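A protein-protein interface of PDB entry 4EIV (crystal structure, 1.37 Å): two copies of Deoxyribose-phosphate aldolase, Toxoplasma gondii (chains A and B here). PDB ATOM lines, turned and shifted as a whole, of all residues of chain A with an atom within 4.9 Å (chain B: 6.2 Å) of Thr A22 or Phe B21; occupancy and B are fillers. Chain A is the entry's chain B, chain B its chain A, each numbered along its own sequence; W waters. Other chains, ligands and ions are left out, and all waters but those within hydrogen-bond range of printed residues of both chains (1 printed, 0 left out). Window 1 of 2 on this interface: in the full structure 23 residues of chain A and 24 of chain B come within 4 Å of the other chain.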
ATOM      1  N   TYR A  18      12.677  15.165   6.633  1.00  0.00           N
ATOM      2  CA  TYR A  18      12.979  14.136   7.615  1.00  0.00           C
ATOM      3  C   TYR A  18      14.424  13.704   7.545  1.00  0.00           C
ATOM      4  O   TYR A  18      15.063  13.514   8.577  1.00  0.00           O
ATOM      5  CB  TYR A  18      12.067  12.942   7.396  1.00  0.00           C
ATOM      6  CG  TYR A  18      10.603  13.307   7.458  1.00  0.00           C
ATOM      7  CD1 TYR A  18      10.004  13.648   8.659  1.00  0.00           C
ATOM      8  CD2 TYR A  18       9.830  13.318   6.312  1.00  0.00           C
ATOM      9  CE1 TYR A  18       8.651  13.995   8.719  1.00  0.00           C
ATOM     10  CE2 TYR A  18       8.460  13.649   6.375  1.00  0.00           C
ATOM     11  CZ  TYR A  18       7.890  13.982   7.584  1.00  0.00           C
ATOM     12  OH  TYR A  18       6.547  14.311   7.672  1.00  0.00           O
ATOM     13  N   LYS A  19      14.944  13.580   6.331  1.00  0.00           N
ATOM     14  CA  LYS A  19      16.363  13.232   6.147  1.00  0.00           C
ATOM     15  C   LYS A  19      17.242  14.395   6.638  1.00  0.00           C
ATOM     16  O   LYS A  19      18.281  14.194   7.264  1.00  0.00           O
ATOM     17  CB  LYS A  19      16.664  12.883   4.685  1.00  0.00           C
ATOM     18  CG  LYS A  19      16.075  11.570   4.267  1.00  0.00           C
ATOM     19  CD  LYS A  19      16.272  11.339   2.770  1.00  0.00           C
ATOM     20  CE  LYS A  19      15.589  10.047   2.282  1.00  0.00           C
ATOM     21  NZ  LYS A  19      15.637   9.921   0.811  1.00  0.00           N
ATOM     22  N   GLN A  20      16.827  15.618   6.325  1.00  0.00           N
ATOM     23  CA  GLN A  20      17.568  16.801   6.755  1.00  0.00           C
ATOM     24  C   GLN A  20      17.619  16.896   8.279  1.00  0.00           C
ATOM     25  O   GLN A  20      18.688  17.179   8.841  1.00  0.00           O
ATOM     26  CB  GLN A  20      16.961  18.053   6.117  1.00  0.00           C
ATOM     27  CG  GLN A  20      17.142  18.087   4.598  1.00  0.00           C
ATOM     28  CD  GLN A  20      16.201  19.029   3.903  1.00  0.00           C
ATOM     29  OE1 GLN A  20      15.171  19.416   4.446  1.00  0.00           O
ATOM     30  NE2 GLN A  20      16.554  19.406   2.683  1.00  0.00           N
ATOM     31  N   PHE A  21      16.488  16.661   8.958  1.00  0.00           N
ATOM     32  CA  PHE A  21      16.470  16.692  10.410  1.00  0.00           C
ATOM     33  C   PHE A  21      17.347  15.576  11.002  1.00  0.00           C
ATOM     34  O   PHE A  21      18.070  15.791  11.978  1.00  0.00           O
ATOM     35  CB  PHE A  21      15.025  16.610  10.944  1.00  0.00           C
ATOM     36  CG  PHE A  21      14.961  16.477  12.426  1.00  0.00           C
ATOM     37  CD1 PHE A  21      15.397  17.492  13.224  1.00  0.00           C
ATOM     38  CD2 PHE A  21      14.485  15.308  13.024  1.00  0.00           C
ATOM     39  CE1 PHE A  21      15.394  17.355  14.604  1.00  0.00           C
ATOM     40  CE2 PHE A  21      14.456  15.187  14.386  1.00  0.00           C
ATOM     41  CZ  PHE A  21      14.905  16.198  15.179  1.00  0.00           C
ATOM     42  N   THR A  22      17.259  14.376  10.443  1.00  0.00           N
ATOM     43  CA  THR A  22      18.044  13.233  10.950  1.00  0.00           C
ATOM     44  C   THR A  22      19.540  13.508  10.782  1.00  0.00           C
ATOM     45  O   THR A  22      20.319  13.273  11.700  1.00  0.00           O
ATOM     46  CB  THR A  22      17.630  11.910  10.254  1.00  0.00           C
ATOM     47  OG1 THR A  22      16.229  11.677  10.480  1.00  0.00           O
ATOM     48  CG2 THR A  22      18.410  10.720  10.814  1.00  0.00           C
ATOM     49  N   SER A  23      19.932  14.004   9.602  1.00  0.00           N
ATOM     50  CA  SER A  23      21.342  14.303   9.353  1.00  0.00           C
ATOM     51  C   SER A  23      21.857  15.415  10.290  1.00  0.00           C
ATOM     52  O   SER A  23      22.977  15.332  10.805  1.00  0.00           O
ATOM     53  CB  SER A  23      21.603  14.618   7.871  1.00  0.00           C
ATOM     54  OG  SER A  23      20.994  15.836   7.470  1.00  0.00           O
ATOM     55  N   ARG A  24      21.041  16.442  10.535  1.00  0.00           N
ATOM     56  CA  ARG A  24      21.435  17.510  11.441  1.00  0.00           C
ATOM     57  C   ARG A  24      21.618  16.999  12.854  1.00  0.00           C
ATOM     58  O   ARG A  24      22.558  17.393  13.556  1.00  0.00           O
ATOM     59  CB  ARG A  24      20.422  18.667  11.412  1.00  0.00           C
ATOM     60  CG  ARG A  24      20.779  19.810  12.338  1.00  0.00           C
ATOM     61  CD  ARG A  24      22.107  20.473  11.957  1.00  0.00           C
ATOM     62  NE  ARG A  24      22.531  21.487  12.916  1.00  0.00           N
ATOM     63  CZ  ARG A  24      23.329  21.293  13.963  1.00  0.00           C
ATOM     64  NH1 ARG A  24      23.796  20.079  14.240  1.00  0.00           N
ATOM     65  NH2 ARG A  24      23.675  22.319  14.715  1.00  0.00           N
ATOM     66  N   THR A  25      20.718  16.107  13.278  1.00  0.00           N
ATOM     67  CA  THR A  25      20.813  15.494  14.606  1.00  0.00           C
ATOM     68  C   THR A  25      22.088  14.639  14.706  1.00  0.00           C
ATOM     69  O   THR A  25      22.849  14.761  15.666  1.00  0.00           O
ATOM     70  CB  THR A  25      19.555  14.631  14.887  1.00  0.00           C
ATOM     71  OG1 THR A  25      18.388  15.471  14.855  1.00  0.00           O
ATOM     72  CG2 THR A  25      19.637  13.943  16.234  1.00  0.00           C
ATOM     73  N   LEU A  26      22.345  13.816  13.691  1.00  0.00           N
ATOM     74  CA  LEU A  26      23.548  12.965  13.689  1.00  0.00           C
ATOM     75  C   LEU A  26      24.824  13.804  13.747  1.00  0.00           C
ATOM     76  O   LEU A  26      25.738  13.461  14.485  1.00  0.00           O
ATOM     77  CB  LEU A  26      23.549  11.985  12.511  1.00  0.00           C
ATOM     78  CG  LEU A  26      22.571  10.816  12.650  1.00  0.00           C
ATOM     79  CD1 LEU A  26      22.367  10.088  11.327  1.00  0.00           C
ATOM     80  CD2 LEU A  26      22.941   9.849  13.802  1.00  0.00           C
ATOM     81  N   ALA A 247      21.064   5.877  11.184  1.00  0.00           N
ATOM     82  CA  ALA A 247      19.792   6.343  11.750  1.00  0.00           C
ATOM     83  C   ALA A 247      19.114   5.233  12.561  1.00  0.00           C
ATOM     84  O   ALA A 247      18.465   5.519  13.567  1.00  0.00           O
ATOM     85  CB  ALA A 247      18.881   6.865  10.643  1.00  0.00           C
ATOM     86  N   LEU A 250      20.501   5.282  15.969  1.00  0.00           N
ATOM     87  CA  LEU A 250      19.936   6.405  16.702  1.00  0.00           C
ATOM     88  C   LEU A 250      18.587   5.995  17.324  1.00  0.00           C
ATOM     89  O   LEU A 250      18.308   6.245  18.501  1.00  0.00           O
ATOM     90  CB  LEU A 250      19.871   7.632  15.800  1.00  0.00           C
ATOM     91  CG  LEU A 250      19.163   8.876  16.267  1.00  0.00           C
ATOM     92  CD1 LEU A 250      19.853   9.397  17.493  1.00  0.00           C
ATOM     93  CD2 LEU A 250      19.158   9.904  15.120  1.00  0.00           C
ATOM     94  N   MET A 251      17.743   5.362  16.520  1.00  0.00           N
ATOM     95  CA  MET A 251      16.468   4.844  16.998  1.00  0.00           C
ATOM     96  C   MET A 251      16.640   3.793  18.108  1.00  0.00           C
ATOM     97  O   MET A 251      15.894   3.795  19.093  1.00  0.00           O
ATOM     98  CB  MET A 251      15.665   4.324  15.821  1.00  0.00           C
ATOM     99  CG  MET A 251      15.047   5.450  15.045  1.00  0.00           C
ATOM    100  SD  MET A 251      13.699   6.265  15.914  1.00  0.00           S
ATOM    101  CE  MET A 251      12.314   5.171  15.632  1.00  0.00           C
ATOM    102  N   ILE A 254      17.450   5.552  21.471  1.00  0.00           N
ATOM    103  CA  ILE A 254      16.269   6.138  22.115  1.00  0.00           C
ATOM    104  C   ILE A 254      15.365   5.061  22.692  1.00  0.00           C
ATOM    105  O   ILE A 254      14.835   5.217  23.772  1.00  0.00           O
ATOM    106  CB  ILE A 254      15.447   6.963  21.113  1.00  0.00           C
ATOM    107  CG1 ILE A 254      16.239   8.167  20.658  1.00  0.00           C
ATOM    108  CG2 ILE A 254      14.121   7.385  21.713  1.00  0.00           C
ATOM    109  CD1 ILE A 254      15.619   8.918  19.540  1.00  0.00           C
ATOM    110  N   THR B  16       9.630   5.344   6.424  1.00  0.00           N
ATOM    111  CA  THR B  16      11.100   5.323   6.403  1.00  0.00           C
ATOM    112  C   THR B  16      11.631   5.455   7.830  1.00  0.00           C
ATOM    113  O   THR B  16      11.011   6.056   8.695  1.00  0.00           O
ATOM    114  CB  THR B  16      11.734   6.463   5.527  1.00  0.00           C
ATOM    115  OG1 THR B  16      11.580   7.759   6.140  1.00  0.00           O
ATOM    116  CG2 THR B  16      11.125   6.480   4.144  1.00  0.00           C
ATOM    117  N   ILE B  17      13.017   5.114   7.976  1.00  0.00           N
ATOM    118  CA  ILE B  17      13.649   5.346   9.264  1.00  0.00           C
ATOM    119  C   ILE B  17      13.655   6.841   9.667  1.00  0.00           C
ATOM    120  O   ILE B  17      13.582   7.174  10.839  1.00  0.00           O
ATOM    121  CB  ILE B  17      15.079   4.731   9.254  1.00  0.00           C
ATOM    122  CG1 ILE B  17      15.702   4.760  10.662  1.00  0.00           C
ATOM    123  CG2 ILE B  17      15.994   5.423   8.227  1.00  0.00           C
ATOM    124  CD1 ILE B  17      14.935   4.032  11.723  1.00  0.00           C
ATOM    125  N   TYR B  18      13.751   7.722   8.683  1.00  0.00           N
ATOM    126  CA  TYR B  18      13.796   9.153   8.901  1.00  0.00           C
ATOM    127  C   TYR B  18      12.480   9.691   9.443  1.00  0.00           C
ATOM    128  O   TYR B  18      12.472  10.493  10.374  1.00  0.00           O
ATOM    129  CB  TYR B  18      14.227   9.867   7.626  1.00  0.00           C
ATOM    130  CG  TYR B  18      15.528   9.310   7.084  1.00  0.00           C
ATOM    131  CD1 TYR B  18      16.720   9.517   7.768  1.00  0.00           C
ATOM    132  CD2 TYR B  18      15.567   8.597   5.885  1.00  0.00           C
ATOM    133  CE1 TYR B  18      17.920   9.014   7.307  1.00  0.00           C
ATOM    134  CE2 TYR B  18      16.778   8.089   5.409  1.00  0.00           C
ATOM    135  CZ  TYR B  18      17.942   8.321   6.129  1.00  0.00           C
ATOM    136  OH  TYR B  18      19.141   7.844   5.664  1.00  0.00           O
ATOM    137  N   LYS B  19      11.372   9.236   8.865  1.00  0.00           N
ATOM    138  CA  LYS B  19      10.059   9.628   9.362  1.00  0.00           C
ATOM    139  C   LYS B  19       9.842   9.037  10.756  1.00  0.00           C
ATOM    140  O   LYS B  19       9.299   9.700  11.622  1.00  0.00           O
ATOM    141  CB  LYS B  19       8.952   9.195   8.395  1.00  0.00           C
ATOM    142  CG  LYS B  19       8.979   9.958   7.079  1.00  0.00           C
ATOM    143  CD  LYS B  19       7.978   9.410   6.063  1.00  0.00           C
ATOM    144  CE  LYS B  19       7.995  10.169   4.741  1.00  0.00           C
ATOM    145  NZ  LYS B  19       7.198   9.473   3.698  1.00  0.00           N
ATOM    146  N   GLN B  20      10.253   7.781  10.948  1.00  0.00           N
ATOM    147  CA  GLN B  20      10.114   7.121  12.247  1.00  0.00           C
ATOM    148  C   GLN B  20      10.882   7.849  13.338  1.00  0.00           C
ATOM    149  O   GLN B  20      10.344   8.052  14.424  1.00  0.00           O
ATOM    150  CB  GLN B  20      10.541   5.657  12.143  1.00  0.00           C
ATOM    151  CG  GLN B  20       9.597   4.823  11.275  1.00  0.00           C
ATOM    152  CD  GLN B  20      10.216   3.542  10.739  1.00  0.00           C
ATOM    153  OE1 GLN B  20      11.422   3.337  10.806  1.00  0.00           O
ATOM    154  NE2 GLN B  20       9.367   2.668  10.206  1.00  0.00           N
ATOM    155  N   PHE B  21      12.092   8.309  13.026  1.00  0.00           N
ATOM    156  CA  PHE B  21      12.888   9.037  14.008  1.00  0.00           C
ATOM    157  C   PHE B  21      12.264  10.403  14.317  1.00  0.00           C
ATOM    158  O   PHE B  21      12.185  10.831  15.462  1.00  0.00           O
ATOM    159  CB  PHE B  21      14.346   9.203  13.549  1.00  0.00           C
ATOM    160  CG  PHE B  21      15.108  10.184  14.385  1.00  0.00           C
ATOM    161  CD1 PHE B  21      15.319   9.957  15.728  1.00  0.00           C
ATOM    162  CD2 PHE B  21      15.558  11.376  13.833  1.00  0.00           C
ATOM    163  CE1 PHE B  21      15.980  10.921  16.499  1.00  0.00           C
ATOM    164  CE2 PHE B  21      16.195  12.309  14.571  1.00  0.00           C
ATOM    165  CZ  PHE B  21      16.402  12.111  15.901  1.00  0.00           C
ATOM    166  N   THR B  22      11.809  11.082  13.282  1.00  0.00           N
ATOM    167  CA  THR B  22      11.177  12.390  13.456  1.00  0.00           C
ATOM    168  C   THR B  22       9.913  12.235  14.278  1.00  0.00           C
ATOM    169  O   THR B  22       9.680  13.028  15.203  1.00  0.00           O
ATOM    170  CB  THR B  22      10.895  13.047  12.089  1.00  0.00           C
ATOM    171  OG1 THR B  22      12.126  13.152  11.384  1.00  0.00           O
ATOM    172  CG2 THR B  22      10.270  14.442  12.245  1.00  0.00           C
ATOM    173  N   SER B  23       9.107  11.220  13.974  1.00  0.00           N
ATOM    174  CA  SER B  23       7.883  10.970  14.746  1.00  0.00           C
ATOM    175  C   SER B  23       8.196  10.706  16.216  1.00  0.00           C
ATOM    176  O   SER B  23       7.545  11.260  17.102  1.00  0.00           O
ATOM    177  CB  SER B  23       7.130   9.769  14.186  1.00  0.00           C
ATOM    178  OG  SER B  23       6.668  10.008  12.872  1.00  0.00           O
ATOM    179  N   ARG B  24       9.206   9.871  16.467  1.00  0.00           N
ATOM    180  CA  ARG B  24       9.592   9.536  17.846  1.00  0.00           C
ATOM    181  C   ARG B  24      10.035  10.770  18.620  1.00  0.00           C
ATOM    182  O   ARG B  24       9.707  10.952  19.790  1.00  0.00           O
ATOM    183  CB  ARG B  24      10.678   8.463  17.864  1.00  0.00           C
ATOM    184  CG  ARG B  24      11.146   8.095  19.275  1.00  0.00           C
ATOM    185  CD  ARG B  24      10.038   7.476  20.104  1.00  0.00           C
ATOM    186  NE  ARG B  24      10.418   7.243  21.493  1.00  0.00           N
ATOM    187  CZ  ARG B  24      10.178   8.068  22.505  1.00  0.00           C
ATOM    188  NH1 ARG B  24       9.605   9.259  22.308  1.00  0.00           N
ATOM    189  NH2 ARG B  24      10.524   7.710  23.724  1.00  0.00           N
ATOM    190  N   THR B  25      10.809  11.612  17.944  1.00  0.00           N
ATOM    191  CA  THR B  25      11.260  12.865  18.499  1.00  0.00           C
ATOM    192  C   THR B  25      10.078  13.771  18.855  1.00  0.00           C
ATOM    193  O   THR B  25      10.018  14.334  19.938  1.00  0.00           O
ATOM    194  CB  THR B  25      12.182  13.585  17.490  1.00  0.00           C
ATOM    195  OG1 THR B  25      13.375  12.813  17.284  1.00  0.00           O
ATOM    196  CG2 THR B  25      12.582  14.973  17.998  1.00  0.00           C
ATOM    197  N   LEU B  26       9.154  13.928  17.927  1.00  0.00           N
ATOM    198  CA  LEU B  26       7.975  14.755  18.186  1.00  0.00           C
ATOM    199  C   LEU B  26       7.116  14.219  19.343  1.00  0.00           C
ATOM    200  O   LEU B  26       6.577  15.006  20.102  1.00  0.00           O
ATOM    201  CB  LEU B  26       7.170  14.954  16.887  1.00  0.00           C
ATOM    202  CG  LEU B  26       7.846  15.875  15.860  1.00  0.00           C
ATOM    203  CD1 LEU B  26       7.222  15.735  14.512  1.00  0.00           C
ATOM    204  CD2 LEU B  26       7.861  17.340  16.325  1.00  0.00           C
ATOM    205  N   MET B 251      13.639  22.045  12.515  1.00  0.00           N
ATOM    206  CA  MET B 251      14.789  22.632  11.839  1.00  0.00           C
ATOM    207  C   MET B 251      14.941  24.108  12.144  1.00  0.00           C
ATOM    208  O   MET B 251      16.065  24.590  12.359  1.00  0.00           O
ATOM    209  CB  MET B 251      14.698  22.409  10.330  1.00  0.00           C
ATOM    210  CG  MET B 251      14.805  20.948   9.947  1.00  0.00           C
ATOM    211  SD  MET B 251      16.365  20.165  10.422  1.00  0.00           S
ATOM    212  CE  MET B 251      17.477  20.732   9.127  1.00  0.00           C
ATOM    213  N   CYS B 282       3.204   6.340  12.757  1.00  0.00           N
ATOM    214  CA  CYS B 282       4.496   6.350  12.101  1.00  0.00           C
ATOM    215  C   CYS B 282       5.539   5.639  12.961  1.00  0.00           C
ATOM    216  O   CYS B 282       6.244   4.746  12.489  1.00  0.00           O
ATOM    217  CB  CYS B 282       4.931   7.784  11.827  1.00  0.00           C
ATOM    218  SG  CYS B 282       6.494   7.899  10.932  1.00  0.00           S
HETATM  219  O   HOH W   1      12.076   5.378  24.487  1.00  0.00           O
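The side-chain sulfur of Met B251 lies close to the backbone NH of Phe A21 (3.8 Å).
The side-chain hydroxyl of Thr B16 lies close to the backbone NH of Tyr B18, 3.3 Å away.
The backbone carbonyl oxygen of Thr B16 sits close to the side-chain amide oxygen of Gln B20, 3.5 Å away.
The side-chain hydroxyl (OG1) of Thr B22 is in hydrogen-bond range of the backbone carbonyl oxygen (O) of Tyr B18.
The backbone NH of Gln B20 sits at hydrogen-bond distance from the side-chain sulfur of Cys B282 (3.8 Å).
O of Gln A20 lies within hydrogen-bond range of OG of Ser A23, 3.0 Å away.
The side-chain hydroxyl (OG1) of Thr A25 lies within hydrogen-bond range of the backbone carbonyl oxygen (O) of Phe A21, at 2.9 Å.
Among the printed residues, merely in contact across the chains: Phe A21 with Phe B21 (3.4 Å), Lys A19 with Tyr B18 (3.4 Å), Thr A22 with Phe B21 (3.4 Å), Met A251 with Phe B21 (3.5 Å), Tyr A18 with Thr B22 (3.5 Å), Thr A22 with Tyr B18 (3.5 Å), Tyr A18 with Lys B19 (3.5 Å), Phe A21 with Thr B22 (3.6 Å), Leu A250 with Phe B21 (3.6 Å), Met A251 with Ile B17 (3.6 Å), Ile A254 with Phe B21 (3.7 Å), Met A251 with Gln B20 (3.7 Å), Ile A254 with Arg B24 (3.7 Å), Thr A25 with Phe B21 (3.7 Å), Gln A20 with Met B251 (3.8 Å), Tyr A18 with Tyr B18 (3.8 Å), Ala A247 with Ile B17 (3.8 Å) and Phe A21 with Thr B25 (3.9 Å).
Of chain B, only Tyr B18 and Phe B21 come within 4 Å of Thr A22.
Phe B21 touches just these residues of chain A: Phe A21 (3.4 Å), Thr A22 (3.4 Å), Thr A25 (3.7 Å), Leu A250 (3.6 Å), Met A251 (3.5 Å) and Ile A254 (3.7 Å).
Of the printed residues of chain B, Met A251 touches Ile B17, Gln B20 and Phe B21.
Of the printed residues of chain A, Met B251 touches Gln A20 and Phe A21.
Of the printed residues of chain B, Gln A20 touches Met B251 (3.8 Å).
Of the printed residues of chain A, Thr B25 touches Phe A21 (3.9 Å).
Cys B282 touches none of the printed residues of chain A.
Of the 13 printed residues of chain B, 9 touch a printed residue of chain A.
Hydrophobic or aromatic side chains of chain A within 4 Å of the printed part of chain B: Tyr A18, Phe A21, Ala A247, Leu A250, Met A251 and Ile A254.
Tyr A18 touches Lys B19, and with the chains exchanged Lys A19 touches Tyr B18.
Gln A20 touches Met B251, and with the chains exchanged Met A251 touches Gln B20.
Phe A21 touches Thr B22, and with the chains exchanged Thr A22 touches Phe B21.
Phe A21 touches Thr B25, and with the chains exchanged Thr A25 touches Phe B21.
Of the 19 pairs that touch across the chains among the printed residues, 14 have their exchanged pair printed and touching as well.
Water W1 bridges the backbone carbonyl oxygen (O) of Ile A254 (2.9 Å) and the guanidinium group (NH2) of Arg B24 (2.9 Å).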
